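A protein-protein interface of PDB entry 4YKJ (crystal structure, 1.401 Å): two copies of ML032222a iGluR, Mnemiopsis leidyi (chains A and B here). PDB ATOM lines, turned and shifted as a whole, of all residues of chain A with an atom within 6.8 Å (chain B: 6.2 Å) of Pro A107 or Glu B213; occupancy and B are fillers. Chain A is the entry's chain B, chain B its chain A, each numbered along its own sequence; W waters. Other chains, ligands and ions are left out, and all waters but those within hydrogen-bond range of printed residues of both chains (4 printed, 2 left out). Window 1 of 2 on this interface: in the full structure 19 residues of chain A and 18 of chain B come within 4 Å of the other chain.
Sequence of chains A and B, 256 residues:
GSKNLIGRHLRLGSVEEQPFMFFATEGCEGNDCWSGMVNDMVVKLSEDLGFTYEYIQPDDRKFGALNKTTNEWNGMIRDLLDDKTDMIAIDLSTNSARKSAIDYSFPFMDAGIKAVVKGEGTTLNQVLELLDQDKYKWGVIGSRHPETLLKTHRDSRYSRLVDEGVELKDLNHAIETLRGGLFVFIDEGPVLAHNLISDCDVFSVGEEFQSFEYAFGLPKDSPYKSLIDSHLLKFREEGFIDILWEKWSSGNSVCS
Hydrophobic or aromatic side chains of chain A within 4 Å of the printed part of chain B: Phe A106 and Pro A107. Of the 15 printed residues of chain B, 5 touch a printed residue of chain A. Printed residues of chain B that touch a printed residue of chain A: Thr B94, Asp B110, Ser B211, Glu B213 and Arg B236. Among the printed residues, Asp or Glu carboxylates within 4 Å of a Lys or Arg side-chain nitrogen of the other chain: Glu A213 with Arg B236 (3.6 Å) and Arg A236 with Glu B213 (3.9 Å).
The side-chain carboxylate of Asp A110 lies close to the side-chain carboxylate of Asp B110, 2.8 Å away. The side-chain carboxylate of Glu A213 is in salt-bridge range of the guanidinium group of Arg B236 (3.6 Å). The side-chain carboxylate (OE2) of Glu B213 lies within salt-bridge range of the guanidinium group (NH1) of Arg A236 (3.9 Å). The side-chain hydroxyl (OG) of Ser B211 sits at hydrogen-bond distance from the guanidinium group (NH2) of Arg A236 (3.4 Å). The side-chain carboxylate (OE2) of Glu A213 sits close to the side-chain carboxylate (OE2) of Glu B213, 3.3 Å away.
N of Thr B94 is in hydrogen-bond range of O of Glu B213, at 2.9 Å. OD2 of Asp B110 lies within salt-bridge range of NH2 of Arg B236 (3.1 Å). The backbone carbonyl oxygen (O) of Pro B107 sits at hydrogen-bond distance from the guanidinium group (NH1) of Arg B236, 3.3 Å away. The backbone carbonyl oxygen (O) of Pro A107 sits at hydrogen-bond distance from the guanidinium group (NH1) of Arg A236, at 3.1 Å. OD1 of Asp A110 lies close to OE1 of Glu A213, at 2.7 Å. The side-chain carboxylate of Asp B110 lies close to the side-chain carboxylate of Glu B213 (2.7 Å).
Water W2 lies within hydrogen-bond range of the side-chain hydroxyl of Ser B211 (2.8 Å) and the guanidinium group of Arg A236 (3.0 Å). Water W1 lies within hydrogen-bond range of the backbone carbonyl oxygen (O) of Arg A236 and the backbone NH (N) of Ser B211. Water W4 lies within hydrogen-bond range of the guanidinium group (NH1) of Arg A236 and the side-chain carboxylate (OE2) of Glu B213. Water W3 lies within hydrogen-bond range of OD2 of Asp B110 and OD2 of Asp A110.
Phe A106 touches Thr B94 (CE1 to CG2, 3.96 Å). Pro A107 touches Glu B213. Asp B110 touches Glu A213 (OD1 to OE2, 3.9 Å).
Asp B110 touches its own counterpart, Asp A110. Glu A213 touches Asp B110, but with the chains exchanged Asp A110 does not touch Glu B213 (4.01 Å). Glu B213 touches its own counterpart, Glu A213. Glu A213 touches Arg B236, and with the chains exchanged Arg A236 touches Glu B213. Positions printed for both chains: 94, 104, 107, 108, 109, 110, 213, 214, 215 and 236.
Pro A107 touches just one residue of chain B: Glu B213 (3.9 Å). Of the printed residues of chain B, Asp A110 touches Asp B110. Of the printed residues of chain B, Phe A106 touches Thr B94. Of the printed residues of chain B, Glu A213 touches Asp B110, Glu B213 and Arg B236. Printed residues of chain A within 4 Å of Asp B110: Asp A110 (2.8 Å) and Glu A213 (3.9 Å). The nearest printed residue of chain A that does not touch Glu B213 is Asp A110 (4.01 Å).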
ATOM      1  N   THR A  94      -7.187 -17.215  12.579  1.00  0.00           N
ATOM      2  CA  THR A  94      -7.941 -16.167  13.267  1.00  0.00           C
ATOM      3  C   THR A  94      -7.012 -15.104  13.847  1.00  0.00           C
ATOM      4  O   THR A  94      -6.107 -15.410  14.630  1.00  0.00           O
ATOM      5  CB  THR A  94      -8.834 -16.763  14.379  1.00  0.00           C
ATOM      6  OG1 THR A  94      -8.023 -17.549  15.274  1.00  0.00           O
ATOM      7  CG2 THR A  94      -9.946 -17.622  13.776  1.00  0.00           C
ATOM      8  N   TYR A 104     -15.345 -15.260  10.504  1.00  0.00           N
ATOM      9  CA  TYR A 104     -14.820 -16.606  10.432  1.00  0.00           C
ATOM     10  C   TYR A 104     -15.906 -17.617  10.650  1.00  0.00           C
ATOM     11  O   TYR A 104     -16.853 -17.381  11.407  1.00  0.00           O
ATOM     12  CB  TYR A 104     -13.773 -16.799  11.507  1.00  0.00           C
ATOM     13  CG  TYR A 104     -12.468 -16.074  11.261  1.00  0.00           C
ATOM     14  CD1 TYR A 104     -11.488 -16.632  10.447  1.00  0.00           C
ATOM     15  CD2 TYR A 104     -12.205 -14.870  11.875  1.00  0.00           C
ATOM     16  CE1 TYR A 104     -10.280 -16.017  10.258  1.00  0.00           C
ATOM     17  CE2 TYR A 104     -10.992 -14.207  11.674  1.00  0.00           C
ATOM     18  CZ  TYR A 104     -10.037 -14.797  10.863  1.00  0.00           C
ATOM     19  OH  TYR A 104      -8.806 -14.183  10.719  1.00  0.00           O
ATOM     20  N   SER A 105     -15.758 -18.770  10.021  1.00  0.00           N
ATOM     21  CA  SER A 105     -16.590 -19.905  10.331  1.00  0.00           C
ATOM     22  C   SER A 105     -16.206 -20.486  11.688  1.00  0.00           C
ATOM     23  O   SER A 105     -15.216 -20.099  12.316  1.00  0.00           O
ATOM     24  CB  SER A 105     -16.400 -20.988   9.272  1.00  0.00           C
ATOM     25  OG  SER A 105     -15.145 -21.630   9.435  1.00  0.00           O
ATOM     26  N   PHE A 106     -16.987 -21.466  12.113  1.00  0.00           N
ATOM     27  CA  PHE A 106     -16.597 -22.328  13.205  1.00  0.00           C
ATOM     28  C   PHE A 106     -15.209 -22.906  12.875  1.00  0.00           C
ATOM     29  O   PHE A 106     -14.950 -23.262  11.730  1.00  0.00           O
ATOM     30  CB  PHE A 106     -17.624 -23.456  13.373  1.00  0.00           C
ATOM     31  CG  PHE A 106     -17.519 -24.152  14.681  1.00  0.00           C
ATOM     32  CD1 PHE A 106     -18.142 -23.627  15.795  1.00  0.00           C
ATOM     33  CD2 PHE A 106     -16.768 -25.301  14.812  1.00  0.00           C
ATOM     34  CE1 PHE A 106     -18.018 -24.222  17.025  1.00  0.00           C
ATOM     35  CE2 PHE A 106     -16.625 -25.911  16.046  1.00  0.00           C
ATOM     36  CZ  PHE A 106     -17.253 -25.360  17.158  1.00  0.00           C
ATOM     37  N   PRO A 107     -14.304 -22.975  13.865  1.00  0.00           N
ATOM     38  CA  PRO A 107     -12.942 -23.455  13.575  1.00  0.00           C
ATOM     39  C   PRO A 107     -12.859 -24.956  13.309  1.00  0.00           C
ATOM     40  O   PRO A 107     -13.676 -25.743  13.834  1.00  0.00           O
ATOM     41  CB  PRO A 107     -12.196 -23.124  14.859  1.00  0.00           C
ATOM     42  CG  PRO A 107     -13.257 -23.213  15.928  1.00  0.00           C
ATOM     43  CD  PRO A 107     -14.469 -22.612  15.284  1.00  0.00           C
ATOM     44  N   PHE A 108     -11.900 -25.361  12.482  1.00  0.00           N
ATOM     45  CA  PHE A 108     -11.637 -26.779  12.259  1.00  0.00           C
ATOM     46  C   PHE A 108     -10.352 -27.320  12.905  1.00  0.00           C
ATOM     47  O   PHE A 108     -10.205 -28.524  13.055  1.00  0.00           O
ATOM     48  CB  PHE A 108     -11.736 -27.143  10.768  1.00  0.00           C
ATOM     49  CG  PHE A 108     -10.634 -26.621   9.882  1.00  0.00           C
ATOM     50  CD1 PHE A 108      -9.493 -27.373   9.669  1.00  0.00           C
ATOM     51  CD2 PHE A 108     -10.771 -25.429   9.177  1.00  0.00           C
ATOM     52  CE1 PHE A 108      -8.497 -26.935   8.826  1.00  0.00           C
ATOM     53  CE2 PHE A 108      -9.781 -25.010   8.318  1.00  0.00           C
ATOM     54  CZ  PHE A 108      -8.647 -25.750   8.144  1.00  0.00           C
ATOM     55  N   MET A 109      -9.444 -26.453  13.338  1.00  0.00           N
ATOM     56  CA  MET A 109      -8.175 -26.914  13.927  1.00  0.00           C
ATOM     57  C   MET A 109      -7.620 -25.843  14.859  1.00  0.00           C
ATOM     58  O   MET A 109      -7.779 -24.662  14.592  1.00  0.00           O
ATOM     59  CB  MET A 109      -7.145 -27.202  12.803  1.00  0.00           C
ATOM     60  CG  MET A 109      -5.847 -27.829  13.279  1.00  0.00           C
ATOM     61  SD  MET A 109      -4.845 -28.420  11.892  1.00  0.00           S
ATOM     62  CE  MET A 109      -5.890 -29.688  11.242  1.00  0.00           C
ATOM     63  N   ASP A 110      -6.954 -26.261  15.930  1.00  0.00           N
ATOM     64  CA  ASP A 110      -6.163 -25.368  16.774  1.00  0.00           C
ATOM     65  C   ASP A 110      -4.739 -25.236  16.236  1.00  0.00           C
ATOM     66  O   ASP A 110      -4.187 -26.182  15.666  1.00  0.00           O
ATOM     67  CB  ASP A 110      -6.134 -25.901  18.199  1.00  0.00           C
ATOM     68  CG  ASP A 110      -7.511 -25.938  18.812  1.00  0.00           C
ATOM     69  OD1 ASP A 110      -8.075 -24.841  19.025  1.00  0.00           O
ATOM     70  OD2 ASP A 110      -8.030 -27.051  19.062  1.00  0.00           O
ATOM     71  N   GLU A 213      -6.881 -20.261  15.866  1.00  0.00           N
ATOM     72  CA  GLU A 213      -7.575 -21.349  15.180  1.00  0.00           C
ATOM     73  C   GLU A 213      -7.416 -21.199  13.695  1.00  0.00           C
ATOM     74  O   GLU A 213      -7.151 -20.114  13.187  1.00  0.00           O
ATOM     75  CB  GLU A 213      -9.076 -21.275  15.463  1.00  0.00           C
ATOM     76  CG  GLU A 213      -9.500 -21.107  16.921  1.00  0.00           C
ATOM     77  CD  GLU A 213      -9.556 -22.408  17.660  1.00  0.00           C
ATOM     78  OE1 GLU A 213      -9.171 -23.430  17.064  1.00  0.00           O
ATOM     79  OE2 GLU A 213      -9.995 -22.412  18.833  1.00  0.00           O
ATOM     80  N   TYR A 214      -7.563 -22.314  12.997  1.00  0.00           N
ATOM     81  CA  TYR A 214      -7.840 -22.305  11.568  1.00  0.00           C
ATOM     82  C   TYR A 214      -9.340 -22.416  11.348  1.00  0.00           C
ATOM     83  O   TYR A 214      -9.992 -23.275  11.943  1.00  0.00           O
ATOM     84  CB  TYR A 214      -7.177 -23.491  10.885  1.00  0.00           C
ATOM     85  CG  TYR A 214      -5.671 -23.479  10.835  1.00  0.00           C
ATOM     86  CD1 TYR A 214      -4.949 -22.292  10.865  1.00  0.00           C
ATOM     87  CD2 TYR A 214      -4.970 -24.662  10.722  1.00  0.00           C
ATOM     88  CE1 TYR A 214      -3.563 -22.312  10.794  1.00  0.00           C
ATOM     89  CE2 TYR A 214      -3.603 -24.690  10.640  1.00  0.00           C
ATOM     90  CZ  TYR A 214      -2.902 -23.531  10.685  1.00  0.00           C
ATOM     91  OH  TYR A 214      -1.527 -23.613  10.592  1.00  0.00           O
ATOM     92  N   ALA A 215      -9.867 -21.576  10.481  1.00  0.00           N
ATOM     93  CA  ALA A 215     -11.269 -21.568  10.131  1.00  0.00           C
ATOM     94  C   ALA A 215     -11.397 -21.193   8.658  1.00  0.00           C
ATOM     95  O   ALA A 215     -10.383 -20.948   7.992  1.00  0.00           O
ATOM     96  CB  ALA A 215     -12.005 -20.581  11.003  1.00  0.00           C
ATOM     97  N   PHE A 216     -12.620 -21.149   8.147  1.00  0.00           N
ATOM     98  CA  PHE A 216     -12.864 -20.590   6.829  1.00  0.00           C
ATOM     99  C   PHE A 216     -13.233 -19.106   7.009  1.00  0.00           C
ATOM    100  O   PHE A 216     -13.762 -18.704   8.056  1.00  0.00           O
ATOM    101  CB  PHE A 216     -13.961 -21.324   6.075  1.00  0.00           C
ATOM    102  CG  PHE A 216     -13.603 -22.729   5.649  1.00  0.00           C
ATOM    103  CD1 PHE A 216     -12.304 -23.221   5.723  1.00  0.00           C
ATOM    104  CD2 PHE A 216     -14.581 -23.555   5.144  1.00  0.00           C
ATOM    105  CE1 PHE A 216     -12.006 -24.529   5.312  1.00  0.00           C
ATOM    106  CE2 PHE A 216     -14.282 -24.853   4.709  1.00  0.00           C
ATOM    107  CZ  PHE A 216     -12.995 -25.324   4.781  1.00  0.00           C
ATOM    108  N   ASP A 229     -21.238 -23.020   9.451  1.00  0.00           N
ATOM    109  CA  ASP A 229     -20.832 -23.221  10.846  1.00  0.00           C
ATOM    110  C   ASP A 229     -21.408 -24.506  11.436  1.00  0.00           C
ATOM    111  O   ASP A 229     -20.710 -25.255  12.098  1.00  0.00           O
ATOM    112  CB  ASP A 229     -21.292 -22.071  11.743  1.00  0.00           C
ATOM    113  CG  ASP A 229     -20.496 -20.791  11.551  1.00  0.00           C
ATOM    114  OD1 ASP A 229     -19.450 -20.859  10.861  1.00  0.00           O
ATOM    115  OD2 ASP A 229     -20.944 -19.754  12.116  1.00  0.00           O
ATOM    116  N   LEU A 232     -19.623 -27.518   9.844  1.00  0.00           N
ATOM    117  CA  LEU A 232     -18.255 -27.666  10.319  1.00  0.00           C
ATOM    118  C   LEU A 232     -18.198 -28.187  11.757  1.00  0.00           C
ATOM    119  O   LEU A 232     -17.325 -28.982  12.117  1.00  0.00           O
ATOM    120  CB  LEU A 232     -17.499 -26.344  10.191  1.00  0.00           C
ATOM    121  CG  LEU A 232     -17.158 -25.962   8.759  1.00  0.00           C
ATOM    122  CD1 LEU A 232     -16.515 -24.576   8.786  1.00  0.00           C
ATOM    123  CD2 LEU A 232     -16.217 -26.960   8.111  1.00  0.00           C
ATOM    124  N   LEU A 233     -19.107 -27.712  12.609  1.00  0.00           N
ATOM    125  CA  LEU A 233     -19.156 -28.203  13.980  1.00  0.00           C
ATOM    126  C   LEU A 233     -19.459 -29.703  13.977  1.00  0.00           C
ATOM    127  O   LEU A 233     -18.836 -30.470  14.699  1.00  0.00           O
ATOM    128  CB  LEU A 233     -20.184 -27.415  14.800  1.00  0.00           C
ATOM    129  CG  LEU A 233     -20.439 -27.864  16.238  1.00  0.00           C
ATOM    130  CD1 LEU A 233     -19.186 -28.140  17.016  1.00  0.00           C
ATOM    131  CD2 LEU A 233     -21.286 -26.798  16.925  1.00  0.00           C
ATOM    132  N   ARG A 236     -16.445 -31.727  13.164  1.00  0.00           N
ATOM    133  CA  ARG A 236     -15.517 -31.840  14.278  1.00  0.00           C
ATOM    134  C   ARG A 236     -16.040 -32.864  15.287  1.00  0.00           C
ATOM    135  O   ARG A 236     -15.308 -33.743  15.740  1.00  0.00           O
ATOM    136  CB  ARG A 236     -15.334 -30.482  14.945  1.00  0.00           C
ATOM    137  CG  ARG A 236     -14.126 -30.418  15.829  1.00  0.00           C
ATOM    138  CD  ARG A 236     -13.002 -29.723  15.100  1.00  0.00           C
ATOM    139  NE  ARG A 236     -11.868 -29.499  15.983  1.00  0.00           N
ATOM    140  CZ  ARG A 236     -11.483 -28.314  16.446  1.00  0.00           C
ATOM    141  NH1 ARG A 236     -12.131 -27.201  16.114  1.00  0.00           N
ATOM    142  NH2 ARG A 236     -10.432 -28.242  17.256  1.00  0.00           N
ATOM    143  N   ILE A 241     -12.773 -34.316  10.991  1.00  0.00           N
ATOM    144  CA  ILE A 241     -11.582 -33.504  10.828  1.00  0.00           C
ATOM    145  C   ILE A 241     -10.341 -34.280  11.255  1.00  0.00           C
ATOM    146  O   ILE A 241      -9.314 -34.237  10.576  1.00  0.00           O
ATOM    147  CB  ILE A 241     -11.687 -32.173  11.593  1.00  0.00           C
ATOM    148  CG1 ILE A 241     -12.928 -31.392  11.143  1.00  0.00           C
ATOM    149  CG2 ILE A 241     -10.423 -31.350  11.383  1.00  0.00           C
ATOM    150  CD1 ILE A 241     -12.996 -31.065   9.652  1.00  0.00           C
ATOM    151  N   LEU B  92     -19.551 -22.705  28.253  1.00  0.00           N
ATOM    152  CA  LEU B  92     -20.643 -23.371  27.540  1.00  0.00           C
ATOM    153  C   LEU B  92     -20.036 -24.167  26.386  1.00  0.00           C
ATOM    154  O   LEU B  92     -19.454 -23.606  25.447  1.00  0.00           O
ATOM    155  CB  LEU B  92     -21.697 -22.389  27.028  1.00  0.00           C
ATOM    156  CG  LEU B  92     -22.997 -23.039  26.556  1.00  0.00           C
ATOM    157  CD1 LEU B  92     -23.776 -23.601  27.727  1.00  0.00           C
ATOM    158  CD2 LEU B  92     -23.820 -22.023  25.761  1.00  0.00           C
ATOM    159  N   SER B  93     -20.131 -25.488  26.484  1.00  0.00           N
ATOM    160  CA  SER B  93     -19.547 -26.359  25.477  1.00  0.00           C
ATOM    161  C   SER B  93     -20.311 -26.311  24.168  1.00  0.00           C
ATOM    162  O   SER B  93     -21.539 -26.240  24.146  1.00  0.00           O
ATOM    163  CB  SER B  93     -19.562 -27.800  25.966  1.00  0.00           C
ATOM    164  OG  SER B  93     -18.798 -27.888  27.159  1.00  0.00           O
ATOM    165  N   THR B  94     -19.560 -26.372  23.075  1.00  0.00           N
ATOM    166  CA  THR B  94     -20.113 -26.460  21.725  1.00  0.00           C
ATOM    167  C   THR B  94     -20.566 -27.876  21.384  1.00  0.00           C
ATOM    168  O   THR B  94     -19.789 -28.816  21.480  1.00  0.00           O
ATOM    169  CB  THR B  94     -19.096 -25.972  20.699  1.00  0.00           C
ATOM    170  OG1 THR B  94     -17.870 -26.696  20.850  1.00  0.00           O
ATOM    171  CG2 THR B  94     -18.832 -24.469  20.896  1.00  0.00           C
ATOM    172  N   TYR B 104     -23.107 -19.531  19.080  1.00  0.00           N
ATOM    173  CA  TYR B 104     -22.003 -19.424  20.012  1.00  0.00           C
ATOM    174  C   TYR B 104     -21.141 -18.239  19.651  1.00  0.00           C
ATOM    175  O   TYR B 104     -21.004 -17.883  18.468  1.00  0.00           O
ATOM    176  CB  TYR B 104     -21.143 -20.665  19.936  1.00  0.00           C
ATOM    177  CG  TYR B 104     -21.744 -21.901  20.538  1.00  0.00           C
ATOM    178  CD1 TYR B 104     -21.676 -22.125  21.909  1.00  0.00           C
ATOM    179  CD2 TYR B 104     -22.343 -22.854  19.749  1.00  0.00           C
ATOM    180  CE1 TYR B 104     -22.175 -23.268  22.469  1.00  0.00           C
ATOM    181  CE2 TYR B 104     -22.875 -24.019  20.313  1.00  0.00           C
ATOM    182  CZ  TYR B 104     -22.792 -24.219  21.667  1.00  0.00           C
ATOM    183  OH  TYR B 104     -23.290 -25.407  22.189  1.00  0.00           O
ATOM    184  N   PRO B 107     -14.785 -18.874  20.534  1.00  0.00           N
ATOM    185  CA  PRO B 107     -14.435 -19.662  21.729  1.00  0.00           C
ATOM    186  C   PRO B 107     -13.322 -19.061  22.582  1.00  0.00           C
ATOM    187  O   PRO B 107     -12.453 -18.332  22.053  1.00  0.00           O
ATOM    188  CB  PRO B 107     -13.969 -20.986  21.147  1.00  0.00           C
ATOM    189  CG  PRO B 107     -13.456 -20.640  19.781  1.00  0.00           C
ATOM    190  CD  PRO B 107     -14.337 -19.524  19.292  1.00  0.00           C
ATOM    191  N   PHE B 108     -13.319 -19.368  23.875  1.00  0.00           N
ATOM    192  CA  PHE B 108     -12.242 -18.930  24.773  1.00  0.00           C
ATOM    193  C   PHE B 108     -11.312 -20.044  25.267  1.00  0.00           C
ATOM    194  O   PHE B 108     -10.251 -19.764  25.803  1.00  0.00           O
ATOM    195  CB  PHE B 108     -12.763 -18.060  25.939  1.00  0.00           C
ATOM    196  CG  PHE B 108     -13.625 -18.772  26.967  1.00  0.00           C
ATOM    197  CD1 PHE B 108     -13.057 -19.328  28.103  1.00  0.00           C
ATOM    198  CD2 PHE B 108     -15.011 -18.765  26.858  1.00  0.00           C
ATOM    199  CE1 PHE B 108     -13.841 -19.932  29.061  1.00  0.00           C
ATOM    200  CE2 PHE B 108     -15.787 -19.349  27.805  1.00  0.00           C
ATOM    201  CZ  PHE B 108     -15.223 -19.931  28.914  1.00  0.00           C
ATOM    202  N   MET B 109     -11.685 -21.300  25.052  1.00  0.00           N
ATOM    203  CA  MET B 109     -10.893 -22.416  25.581  1.00  0.00           C
ATOM    204  C   MET B 109     -11.223 -23.683  24.816  1.00  0.00           C
ATOM    205  O   MET B 109     -12.364 -23.871  24.432  1.00  0.00           O
ATOM    206  CB  MET B 109     -11.242 -22.649  27.069  1.00  0.00           C
ATOM    207  CG  MET B 109     -10.342 -23.646  27.759  1.00  0.00           C
ATOM    208  SD  MET B 109     -10.541 -23.597  29.553  1.00  0.00           S
ATOM    209  CE  MET B 109      -9.946 -21.975  29.943  1.00  0.00           C
ATOM    210  N   ASP B 110     -10.236 -24.552  24.623  1.00  0.00           N
ATOM    211  CA  ASP B 110     -10.435 -25.902  24.096  1.00  0.00           C
ATOM    212  C   ASP B 110     -10.705 -26.875  25.236  1.00  0.00           C
ATOM    213  O   ASP B 110     -10.217 -26.690  26.352  1.00  0.00           O
ATOM    214  CB  ASP B 110      -9.201 -26.342  23.301  1.00  0.00           C
ATOM    215  CG  ASP B 110      -8.950 -25.445  22.118  1.00  0.00           C
ATOM    216  OD1 ASP B 110      -9.766 -25.507  21.174  1.00  0.00           O
ATOM    217  OD2 ASP B 110      -7.965 -24.670  22.134  1.00  0.00           O
ATOM    218  N   ALA B 111     -11.502 -27.896  24.974  1.00  0.00           N
ATOM    219  CA  ALA B 111     -11.822 -28.871  25.998  1.00  0.00           C
ATOM    220  C   ALA B 111     -12.138 -30.232  25.397  1.00  0.00           C
ATOM    221  O   ALA B 111     -12.499 -30.349  24.232  1.00  0.00           O
ATOM    222  CB  ALA B 111     -12.992 -28.385  26.833  1.00  0.00           C
ATOM    223  N   SER B 211     -13.178 -33.423  20.634  1.00  0.00           N
ATOM    224  CA  SER B 211     -12.662 -32.074  20.739  1.00  0.00           C
ATOM    225  C   SER B 211     -13.819 -31.108  20.613  1.00  0.00           C
ATOM    226  O   SER B 211     -14.593 -31.197  19.679  1.00  0.00           O
ATOM    227  CB  SER B 211     -11.651 -31.836  19.610  1.00  0.00           C
ATOM    228  OG  SER B 211     -11.088 -30.544  19.684  1.00  0.00           O
ATOM    229  N   PHE B 212     -13.965 -30.200  21.577  1.00  0.00           N
ATOM    230  CA  PHE B 212     -14.948 -29.127  21.478  1.00  0.00           C
ATOM    231  C   PHE B 212     -14.386 -27.872  22.141  1.00  0.00           C
ATOM    232  O   PHE B 212     -13.210 -27.844  22.513  1.00  0.00           O
ATOM    233  CB  PHE B 212     -16.288 -29.572  22.082  1.00  0.00           C
ATOM    234  CG  PHE B 212     -16.172 -30.089  23.488  1.00  0.00           C
ATOM    235  CD1 PHE B 212     -15.909 -31.429  23.719  1.00  0.00           C
ATOM    236  CD2 PHE B 212     -16.295 -29.247  24.575  1.00  0.00           C
ATOM    237  CE1 PHE B 212     -15.778 -31.913  25.006  1.00  0.00           C
ATOM    238  CE2 PHE B 212     -16.170 -29.722  25.870  1.00  0.00           C
ATOM    239  CZ  PHE B 212     -15.917 -31.060  26.085  1.00  0.00           C
ATOM    240  N   GLU B 213     -15.208 -26.842  22.217  1.00  0.00           N
ATOM    241  CA  GLU B 213     -14.784 -25.542  22.721  1.00  0.00           C
ATOM    242  C   GLU B 213     -15.703 -25.077  23.817  1.00  0.00           C
ATOM    243  O   GLU B 213     -16.866 -25.489  23.888  1.00  0.00           O
ATOM    244  CB  GLU B 213     -14.861 -24.485  21.598  1.00  0.00           C
ATOM    245  CG  GLU B 213     -14.216 -24.848  20.272  1.00  0.00           C
ATOM    246  CD  GLU B 213     -12.724 -24.657  20.285  1.00  0.00           C
ATOM    247  OE1 GLU B 213     -12.195 -24.240  21.337  1.00  0.00           O
ATOM    248  OE2 GLU B 213     -12.077 -24.917  19.241  1.00  0.00           O
ATOM    249  N   TYR B 214     -15.191 -24.189  24.667  1.00  0.00           N
ATOM    250  CA  TYR B 214     -16.021 -23.392  25.540  1.00  0.00           C
ATOM    251  C   TYR B 214     -16.195 -22.029  24.892  1.00  0.00           C
ATOM    252  O   TYR B 214     -15.213 -21.437  24.395  1.00  0.00           O
ATOM    253  CB  TYR B 214     -15.385 -23.192  26.909  1.00  0.00           C
ATOM    254  CG  TYR B 214     -15.269 -24.416  27.803  1.00  0.00           C
ATOM    255  CD1 TYR B 214     -16.152 -25.478  27.706  1.00  0.00           C
ATOM    256  CD2 TYR B 214     -14.269 -24.489  28.752  1.00  0.00           C
ATOM    257  CE1 TYR B 214     -16.032 -26.564  28.548  1.00  0.00           C
ATOM    258  CE2 TYR B 214     -14.156 -25.557  29.586  1.00  0.00           C
ATOM    259  CZ  TYR B 214     -15.041 -26.587  29.500  1.00  0.00           C
ATOM    260  OH  TYR B 214     -14.906 -27.656  30.363  1.00  0.00           O
ATOM    261  N   ALA B 215     -17.436 -21.542  24.891  1.00  0.00           N
ATOM    262  CA  ALA B 215     -17.778 -20.261  24.297  1.00  0.00           C
ATOM    263  C   ALA B 215     -18.915 -19.698  25.114  1.00  0.00           C
ATOM    264  O   ALA B 215     -19.361 -20.337  26.067  1.00  0.00           O
ATOM    265  CB  ALA B 215     -18.208 -20.445  22.820  1.00  0.00           C
ATOM    266  N   ARG B 236      -8.131 -13.446  23.544  1.00  0.00           N
ATOM    267  CA  ARG B 236      -7.307 -14.614  23.361  1.00  0.00           C
ATOM    268  C   ARG B 236      -5.966 -14.216  22.752  1.00  0.00           C
ATOM    269  O   ARG B 236      -4.909 -14.641  23.230  1.00  0.00           O
ATOM    270  CB  ARG B 236      -8.017 -15.641  22.503  1.00  0.00           C
ATOM    271  CG  ARG B 236      -7.437 -17.015  22.665  1.00  0.00           C
ATOM    272  CD  ARG B 236      -8.434 -18.061  22.246  1.00  0.00           C
ATOM    273  NE  ARG B 236      -8.011 -19.386  22.680  1.00  0.00           N
ATOM    274  CZ  ARG B 236      -8.707 -20.495  22.460  1.00  0.00           C
ATOM    275  NH1 ARG B 236      -9.866 -20.431  21.819  1.00  0.00           N
ATOM    276  NH2 ARG B 236      -8.245 -21.665  22.882  1.00  0.00           N
HETATM  277  O   HOH W   1     -14.151 -34.679  18.165  1.00  0.00           O
HETATM  278  O   HOH W   2      -8.755 -30.630  18.111  1.00  0.00           O
HETATM  279  O   HOH W   3      -6.170 -27.145  21.722  1.00  0.00           O
HETATM  280  O   HOH W   4     -13.062 -27.756  18.868  1.00  0.00           O
